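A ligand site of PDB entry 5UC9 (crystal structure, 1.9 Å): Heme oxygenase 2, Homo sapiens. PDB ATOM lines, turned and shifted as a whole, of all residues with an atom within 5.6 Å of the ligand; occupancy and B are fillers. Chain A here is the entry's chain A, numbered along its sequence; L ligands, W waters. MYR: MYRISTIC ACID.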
ATOM      1  N   PHE A  37      19.704 -23.353 -18.085  1.00  0.00           N
ATOM      2  CA  PHE A  37      20.913 -22.571 -18.316  1.00  0.00           C
ATOM      3  C   PHE A  37      20.990 -21.378 -17.372  1.00  0.00           C
ATOM      4  O   PHE A  37      22.056 -21.081 -16.821  1.00  0.00           O
ATOM      5  CB  PHE A  37      20.993 -22.099 -19.765  1.00  0.00           C
ATOM      6  CG  PHE A  37      22.171 -21.214 -20.031  1.00  0.00           C
ATOM      7  CD1 PHE A  37      23.405 -21.773 -20.328  1.00  0.00           C
ATOM      8  CD2 PHE A  37      22.065 -19.830 -19.938  1.00  0.00           C
ATOM      9  CE1 PHE A  37      24.501 -20.962 -20.562  1.00  0.00           C
ATOM     10  CE2 PHE A  37      23.161 -19.019 -20.171  1.00  0.00           C
ATOM     11  CZ  PHE A  37      24.380 -19.590 -20.484  1.00  0.00           C
ATOM     12  N   VAL A  38      19.869 -20.669 -17.188  1.00  0.00           N
ATOM     13  CA  VAL A  38      19.876 -19.508 -16.314  1.00  0.00           C
ATOM     14  C   VAL A  38      20.120 -19.919 -14.868  1.00  0.00           C
ATOM     15  O   VAL A  38      20.902 -19.286 -14.136  1.00  0.00           O
ATOM     16  CB  VAL A  38      18.562 -18.721 -16.447  1.00  0.00           C
ATOM     17  CG1 VAL A  38      18.538 -17.590 -15.451  1.00  0.00           C
ATOM     18  CG2 VAL A  38      18.390 -18.206 -17.869  1.00  0.00           C
ATOM     19  N   PHE A  41      23.769 -20.833 -14.519  1.00  0.00           N
ATOM     20  CA  PHE A  41      24.639 -19.669 -14.567  1.00  0.00           C
ATOM     21  C   PHE A  41      24.656 -18.932 -13.236  1.00  0.00           C
ATOM     22  O   PHE A  41      25.723 -18.647 -12.678  1.00  0.00           O
ATOM     23  CB  PHE A  41      24.189 -18.720 -15.679  1.00  0.00           C
ATOM     24  CG  PHE A  41      24.973 -17.446 -15.718  1.00  0.00           C
ATOM     25  CD1 PHE A  41      26.171 -17.386 -16.413  1.00  0.00           C
ATOM     26  CD2 PHE A  41      24.543 -16.317 -15.031  1.00  0.00           C
ATOM     27  CE1 PHE A  41      26.917 -16.223 -16.431  1.00  0.00           C
ATOM     28  CE2 PHE A  41      25.291 -15.152 -15.058  1.00  0.00           C
ATOM     29  CZ  PHE A  41      26.469 -15.099 -15.748  1.00  0.00           C
ATOM     30  N   PHE A  51      30.124 -20.507 -21.864  1.00  0.00           N
ATOM     31  CA  PHE A  51      29.940 -19.058 -21.791  1.00  0.00           C
ATOM     32  C   PHE A  51      30.392 -18.367 -23.086  1.00  0.00           C
ATOM     33  O   PHE A  51      29.810 -17.347 -23.488  1.00  0.00           O
ATOM     34  CB  PHE A  51      30.702 -18.522 -20.585  1.00  0.00           C
ATOM     35  CG  PHE A  51      30.413 -17.081 -20.282  1.00  0.00           C
ATOM     36  CD1 PHE A  51      29.254 -16.722 -19.611  1.00  0.00           C
ATOM     37  CD2 PHE A  51      31.285 -16.091 -20.680  1.00  0.00           C
ATOM     38  CE1 PHE A  51      28.981 -15.374 -19.357  1.00  0.00           C
ATOM     39  CE2 PHE A  51      31.025 -14.750 -20.426  1.00  0.00           C
ATOM     40  CZ  PHE A  51      29.870 -14.398 -19.766  1.00  0.00           C
ATOM     41  N   ALA A  54      27.480 -18.769 -25.400  1.00  0.00           N
ATOM     42  CA  ALA A  54      26.402 -17.850 -25.058  1.00  0.00           C
ATOM     43  C   ALA A  54      26.750 -16.434 -25.493  1.00  0.00           C
ATOM     44  O   ALA A  54      25.897 -15.678 -25.969  1.00  0.00           O
ATOM     45  CB  ALA A  54      26.128 -17.904 -23.548  1.00  0.00           C
ATOM     46  N   THR A  55      28.025 -16.074 -25.370  1.00  0.00           N
ATOM     47  CA  THR A  55      28.495 -14.742 -25.772  1.00  0.00           C
ATOM     48  C   THR A  55      28.464 -14.581 -27.289  1.00  0.00           C
ATOM     49  O   THR A  55      28.089 -13.516 -27.812  1.00  0.00           O
ATOM     50  CB  THR A  55      29.897 -14.523 -25.202  1.00  0.00           C
ATOM     51  OG1 THR A  55      29.846 -14.665 -23.767  1.00  0.00           O
ATOM     52  CG2 THR A  55      30.411 -13.135 -25.541  1.00  0.00           C
ATOM     53  N   ALA A  57      26.271 -16.002 -29.197  1.00  0.00           N
ATOM     54  CA  ALA A  57      24.865 -15.767 -29.511  1.00  0.00           C
ATOM     55  C   ALA A  57      24.485 -14.309 -29.292  1.00  0.00           C
ATOM     56  O   ALA A  57      23.764 -13.710 -30.103  1.00  0.00           O
ATOM     57  CB  ALA A  57      23.985 -16.704 -28.686  1.00  0.00           C
ATOM     58  N   LEU A  58      24.979 -13.699 -28.209  1.00  0.00           N
ATOM     59  CA  LEU A  58      24.701 -12.288 -27.963  1.00  0.00           C
ATOM     60  C   LEU A  58      25.317 -11.412 -29.043  1.00  0.00           C
ATOM     61  O   LEU A  58      24.713 -10.435 -29.480  1.00  0.00           O
ATOM     62  CB  LEU A  58      25.244 -11.870 -26.592  1.00  0.00           C
ATOM     63  CG  LEU A  58      24.579 -12.500 -25.361  1.00  0.00           C
ATOM     64  CD1 LEU A  58      25.410 -12.228 -24.098  1.00  0.00           C
ATOM     65  CD2 LEU A  58      23.161 -11.966 -25.205  1.00  0.00           C
ATOM     66  N   THR A  61      23.174 -11.566 -32.074  1.00  0.00           N
ATOM     67  CA  THR A  61      21.877 -10.976 -31.770  1.00  0.00           C
ATOM     68  C   THR A  61      21.960  -9.457 -31.739  1.00  0.00           C
ATOM     69  O   THR A  61      21.157  -8.772 -32.389  1.00  0.00           O
ATOM     70  CB  THR A  61      21.353 -11.485 -30.425  1.00  0.00           C
ATOM     71  OG1 THR A  61      21.092 -12.891 -30.514  1.00  0.00           O
ATOM     72  CG2 THR A  61      20.059 -10.735 -30.054  1.00  0.00           C
ATOM     73  N   TYR A 118      16.429 -16.139 -34.344  1.00  0.00           N
ATOM     74  CA  TYR A 118      16.104 -14.843 -33.758  1.00  0.00           C
ATOM     75  C   TYR A 118      16.657 -13.707 -34.604  1.00  0.00           C
ATOM     76  O   TYR A 118      15.966 -12.708 -34.832  1.00  0.00           O
ATOM     77  CB  TYR A 118      16.634 -14.779 -32.323  1.00  0.00           C
ATOM     78  CG  TYR A 118      16.208 -13.508 -31.593  1.00  0.00           C
ATOM     79  CD1 TYR A 118      14.891 -13.101 -31.624  1.00  0.00           C
ATOM     80  CD2 TYR A 118      17.114 -12.738 -30.871  1.00  0.00           C
ATOM     81  CE1 TYR A 118      14.480 -11.939 -30.968  1.00  0.00           C
ATOM     82  CE2 TYR A 118      16.716 -11.583 -30.214  1.00  0.00           C
ATOM     83  CZ  TYR A 118      15.384 -11.189 -30.261  1.00  0.00           C
ATOM     84  OH  TYR A 118      14.958 -10.042 -29.611  1.00  0.00           O
ATOM     85  N   HIS A 136      11.558  -5.640 -29.326  1.00  0.00           N
ATOM     86  CA  HIS A 136      12.860  -6.268 -29.150  1.00  0.00           C
ATOM     87  C   HIS A 136      13.831  -5.364 -28.408  1.00  0.00           C
ATOM     88  O   HIS A 136      14.604  -5.837 -27.560  1.00  0.00           O
ATOM     89  CB  HIS A 136      13.442  -6.651 -30.507  1.00  0.00           C
ATOM     90  CG  HIS A 136      12.690  -7.767 -31.155  1.00  0.00           C
ATOM     91  ND1 HIS A 136      12.831  -9.075 -30.757  1.00  0.00           N
ATOM     92  CD2 HIS A 136      11.774  -7.773 -32.144  1.00  0.00           C
ATOM     93  CE1 HIS A 136      12.041  -9.840 -31.479  1.00  0.00           C
ATOM     94  NE2 HIS A 136      11.381  -9.075 -32.336  1.00  0.00           N
ATOM     95  N   THR A 139      12.737  -5.147 -24.568  1.00  0.00           N
ATOM     96  CA  THR A 139      12.968  -6.395 -23.851  1.00  0.00           C
ATOM     97  C   THR A 139      14.449  -6.665 -23.636  1.00  0.00           C
ATOM     98  O   THR A 139      14.845  -7.127 -22.550  1.00  0.00           O
ATOM     99  CB  THR A 139      12.317  -7.543 -24.624  1.00  0.00           C
ATOM    100  OG1 THR A 139      10.933  -7.240 -24.794  1.00  0.00           O
ATOM    101  CG2 THR A 139      12.439  -8.837 -23.843  1.00  0.00           C
ATOM    102  N   ARG A 140      15.284  -6.412 -24.642  1.00  0.00           N
ATOM    103  CA  ARG A 140      16.709  -6.670 -24.476  1.00  0.00           C
ATOM    104  C   ARG A 140      17.344  -5.627 -23.553  1.00  0.00           C
ATOM    105  O   ARG A 140      17.918  -5.973 -22.503  1.00  0.00           O
ATOM    106  CB  ARG A 140      17.418  -6.706 -25.827  1.00  0.00           C
ATOM    107  CG  ARG A 140      17.228  -8.032 -26.633  1.00  0.00           C
ATOM    108  CD  ARG A 140      17.398  -9.304 -25.766  1.00  0.00           C
ATOM    109  NE  ARG A 140      18.631  -9.314 -24.975  1.00  0.00           N
ATOM    110  CZ  ARG A 140      19.044 -10.331 -24.217  1.00  0.00           C
ATOM    111  NH1 ARG A 140      18.331 -11.442 -24.130  1.00  0.00           N
ATOM    112  NH2 ARG A 140      20.184 -10.225 -23.530  1.00  0.00           N
ATOM    113  N   LEU A 151      24.961  -9.986 -13.245  1.00  0.00           N
ATOM    114  CA  LEU A 151      25.476 -11.008 -14.154  1.00  0.00           C
ATOM    115  C   LEU A 151      26.985 -10.896 -14.327  1.00  0.00           C
ATOM    116  O   LEU A 151      27.679 -11.917 -14.405  1.00  0.00           O
ATOM    117  CB  LEU A 151      24.776 -10.917 -15.500  1.00  0.00           C
ATOM    118  CG  LEU A 151      23.261 -11.097 -15.447  1.00  0.00           C
ATOM    119  CD1 LEU A 151      22.704 -11.061 -16.885  1.00  0.00           C
ATOM    120  CD2 LEU A 151      22.924 -12.425 -14.752  1.00  0.00           C
ATOM    121  N   TYR A 171      28.169  -6.276 -20.095  1.00  0.00           N
ATOM    122  CA  TYR A 171      27.307  -6.065 -18.928  1.00  0.00           C
ATOM    123  C   TYR A 171      27.473  -4.683 -18.311  1.00  0.00           C
ATOM    124  O   TYR A 171      26.699  -4.336 -17.411  1.00  0.00           O
ATOM    125  CB  TYR A 171      27.594  -7.170 -17.890  1.00  0.00           C
ATOM    126  CG  TYR A 171      27.353  -8.552 -18.457  1.00  0.00           C
ATOM    127  CD1 TYR A 171      26.061  -9.100 -18.510  1.00  0.00           C
ATOM    128  CD2 TYR A 171      28.391  -9.286 -19.025  1.00  0.00           C
ATOM    129  CE1 TYR A 171      25.825 -10.355 -19.070  1.00  0.00           C
ATOM    130  CE2 TYR A 171      28.159 -10.537 -19.603  1.00  0.00           C
ATOM    131  CZ  TYR A 171      26.874 -11.067 -19.620  1.00  0.00           C
ATOM    132  OH  TYR A 171      26.638 -12.322 -20.179  1.00  0.00           O
ATOM    133  N   ALA A 210       9.905 -12.658 -28.599  1.00  0.00           N
ATOM    134  CA  ALA A 210      11.316 -12.515 -28.253  1.00  0.00           C
ATOM    135  C   ALA A 210      11.702 -13.381 -27.060  1.00  0.00           C
ATOM    136  O   ALA A 210      12.769 -14.010 -27.059  1.00  0.00           O
ATOM    137  CB  ALA A 210      11.630 -11.040 -27.974  1.00  0.00           C
ATOM    138  N   PHE A 211      10.846 -13.421 -26.032  1.00  0.00           N
ATOM    139  CA  PHE A 211      11.151 -14.263 -24.879  1.00  0.00           C
ATOM    140  C   PHE A 211      11.189 -15.725 -25.272  1.00  0.00           C
ATOM    141  O   PHE A 211      11.927 -16.518 -24.667  1.00  0.00           O
ATOM    142  CB  PHE A 211      10.128 -14.041 -23.769  1.00  0.00           C
ATOM    143  CG  PHE A 211      10.452 -12.903 -22.857  1.00  0.00           C
ATOM    144  CD1 PHE A 211      11.466 -13.017 -21.919  1.00  0.00           C
ATOM    145  CD2 PHE A 211       9.762 -11.714 -22.949  1.00  0.00           C
ATOM    146  CE1 PHE A 211      11.776 -11.955 -21.089  1.00  0.00           C
ATOM    147  CE2 PHE A 211      10.061 -10.656 -22.111  1.00  0.00           C
ATOM    148  CZ  PHE A 211      11.068 -10.771 -21.185  1.00  0.00           C
ATOM    149  N   TYR A 213      12.183 -16.968 -28.380  1.00  0.00           N
ATOM    150  CA  TYR A 213      13.522 -17.109 -28.941  1.00  0.00           C
ATOM    151  C   TYR A 213      14.575 -17.154 -27.835  1.00  0.00           C
ATOM    152  O   TYR A 213      15.511 -17.967 -27.877  1.00  0.00           O
ATOM    153  CB  TYR A 213      13.808 -15.972 -29.916  1.00  0.00           C
ATOM    154  CG  TYR A 213      13.057 -16.072 -31.230  1.00  0.00           C
ATOM    155  CD1 TYR A 213      13.378 -17.068 -32.156  1.00  0.00           C
ATOM    156  CD2 TYR A 213      12.053 -15.166 -31.554  1.00  0.00           C
ATOM    157  CE1 TYR A 213      12.688 -17.167 -33.366  1.00  0.00           C
ATOM    158  CE2 TYR A 213      11.372 -15.262 -32.762  1.00  0.00           C
ATOM    159  CZ  TYR A 213      11.688 -16.265 -33.659  1.00  0.00           C
ATOM    160  OH  TYR A 213      11.011 -16.339 -34.861  1.00  0.00           O
ATOM    161  N   ASN A 214      14.410 -16.293 -26.830  1.00  0.00           N
ATOM    162  CA  ASN A 214      15.264 -16.296 -25.655  1.00  0.00           C
ATOM    163  C   ASN A 214      15.341 -17.672 -25.035  1.00  0.00           C
ATOM    164  O   ASN A 214      16.421 -18.196 -24.759  1.00  0.00           O
ATOM    165  CB  ASN A 214      14.717 -15.279 -24.650  1.00  0.00           C
ATOM    166  CG  ASN A 214      15.698 -14.911 -23.548  1.00  0.00           C
ATOM    167  OD1 ASN A 214      16.877 -14.642 -23.815  1.00  0.00           O
ATOM    168  ND2 ASN A 214      15.214 -14.889 -22.317  1.00  0.00           N
ATOM    169  N   ILE A 217      17.168 -20.157 -27.281  1.00  0.00           N
ATOM    170  CA  ILE A 217      18.621 -20.041 -27.266  1.00  0.00           C
ATOM    171  C   ILE A 217      19.195 -20.648 -25.994  1.00  0.00           C
ATOM    172  O   ILE A 217      20.196 -21.386 -26.039  1.00  0.00           O
ATOM    173  CB  ILE A 217      19.044 -18.570 -27.447  1.00  0.00           C
ATOM    174  CG1 ILE A 217      18.585 -18.057 -28.824  1.00  0.00           C
ATOM    175  CG2 ILE A 217      20.567 -18.419 -27.318  1.00  0.00           C
ATOM    176  CD1 ILE A 217      18.740 -16.559 -28.982  1.00  0.00           C
ATOM    177  N   PHE A 218      18.571 -20.372 -24.834  1.00  0.00           N
ATOM    178  CA  PHE A 218      18.996 -20.970 -23.575  1.00  0.00           C
ATOM    179  C   PHE A 218      19.000 -22.496 -23.655  1.00  0.00           C
ATOM    180  O   PHE A 218      19.948 -23.160 -23.236  1.00  0.00           O
ATOM    181  CB  PHE A 218      18.063 -20.524 -22.431  1.00  0.00           C
ATOM    182  CG  PHE A 218      18.309 -19.108 -21.927  1.00  0.00           C
ATOM    183  CD1 PHE A 218      19.596 -18.607 -21.792  1.00  0.00           C
ATOM    184  CD2 PHE A 218      17.247 -18.292 -21.574  1.00  0.00           C
ATOM    185  CE1 PHE A 218      19.810 -17.296 -21.297  1.00  0.00           C
ATOM    186  CE2 PHE A 218      17.447 -16.991 -21.104  1.00  0.00           C
ATOM    187  CZ  PHE A 218      18.734 -16.490 -20.969  1.00  0.00           C
ATOM    188  N   LEU A 221      21.795 -23.805 -25.649  1.00  0.00           N
ATOM    189  CA  LEU A 221      23.009 -23.758 -24.849  1.00  0.00           C
ATOM    190  C   LEU A 221      23.058 -24.901 -23.839  1.00  0.00           C
ATOM    191  O   LEU A 221      24.123 -25.485 -23.610  1.00  0.00           O
ATOM    192  CB  LEU A 221      23.118 -22.424 -24.117  1.00  0.00           C
ATOM    193  CG  LEU A 221      23.396 -21.284 -25.062  1.00  0.00           C
ATOM    194  CD1 LEU A 221      23.169 -19.973 -24.320  1.00  0.00           C
ATOM    195  CD2 LEU A 221      24.821 -21.410 -25.552  1.00  0.00           C
HETATM  196  C1  MYR L   1      16.372 -12.614 -26.514  1.00  0.00           C
HETATM  197  O1  MYR L   1      15.558 -12.554 -25.560  1.00  0.00           O
HETATM  198  O2  MYR L   1      16.246 -11.731 -27.388  1.00  0.00           O
HETATM  199  C2  MYR L   1      17.457 -13.689 -26.609  1.00  0.00           C
HETATM  200  C3  MYR L   1      18.879 -13.184 -26.377  1.00  0.00           C
HETATM  201  C4  MYR L   1      19.929 -14.277 -26.119  1.00  0.00           C
HETATM  202  C5  MYR L   1      19.736 -15.008 -24.788  1.00  0.00           C
HETATM  203  C6  MYR L   1      20.922 -15.867 -24.340  1.00  0.00           C
HETATM  204  C7  MYR L   1      21.934 -15.044 -23.547  1.00  0.00           C
HETATM  205  C8  MYR L   1      23.062 -15.846 -22.919  1.00  0.00           C
HETATM  206  C9  MYR L   1      23.844 -14.996 -21.899  1.00  0.00           C
HETATM  207  C10 MYR L   1      23.694 -15.448 -20.447  1.00  0.00           C
HETATM  208  C11 MYR L   1      22.858 -14.485 -19.596  1.00  0.00           C
HETATM  209  C12 MYR L   1      22.064 -15.245 -18.531  1.00  0.00           C
HETATM  210  C13 MYR L   1      21.226 -14.355 -17.634  1.00  0.00           C
HETATM  211  C14 MYR L   1      19.907 -13.870 -18.251  1.00  0.00           C
HETATM  212  O   HOH W   1      15.431 -10.529 -22.948  1.00  0.00           O
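The side-chain hydroxyl (OH) of Tyr 118 lies close to an oxygen (O2) of the ligand, 3.1 Å away. The guanidinium group (NH1) of Arg 140 lies within salt-bridge range of an oxygen (O1) of the ligand, 3.3 Å away. An oxygen (O1) of the ligand sits close to the side-chain amide oxygen of Asn 214, at 3.0 Å.
OH of Tyr 118 sits at hydrogen-bond distance from ND1 of His 136, 2.6 Å away.
O1 of the ligand sits close to O of Ala 210, 3.5 Å away. CE2 of Phe 37 touches C10 of the ligand, 3.6 Å away. CB of Ala 54 touches C8 of the ligand, 3.7 Å away. Leu 58 touches the ligand (CD2 to C7, 3.7 Å). Leu 151 touches the ligand (CD1 to C13, 3.7 Å). Ile 217 touches the ligand (CD1 to C4, 3.8 Å). CE1 of Phe 218 touches C6 of the ligand, 3.5 Å away. Hydrophobic or aromatic side chains that line the ligand: Phe 37, Ala 54, Leu 58, Tyr 118, Leu 151, Ile 217 and Phe 218. The nearest printed residue that does not touch the ligand is Tyr 171 (4.2 Å).
Water W1 lies within hydrogen-bond range of the guanidinium group of Arg 140 (3.3 Å), an oxygen (O1) of the ligand (3.3 Å) and the backbone carbonyl oxygen of Thr 139 (3.5 Å).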
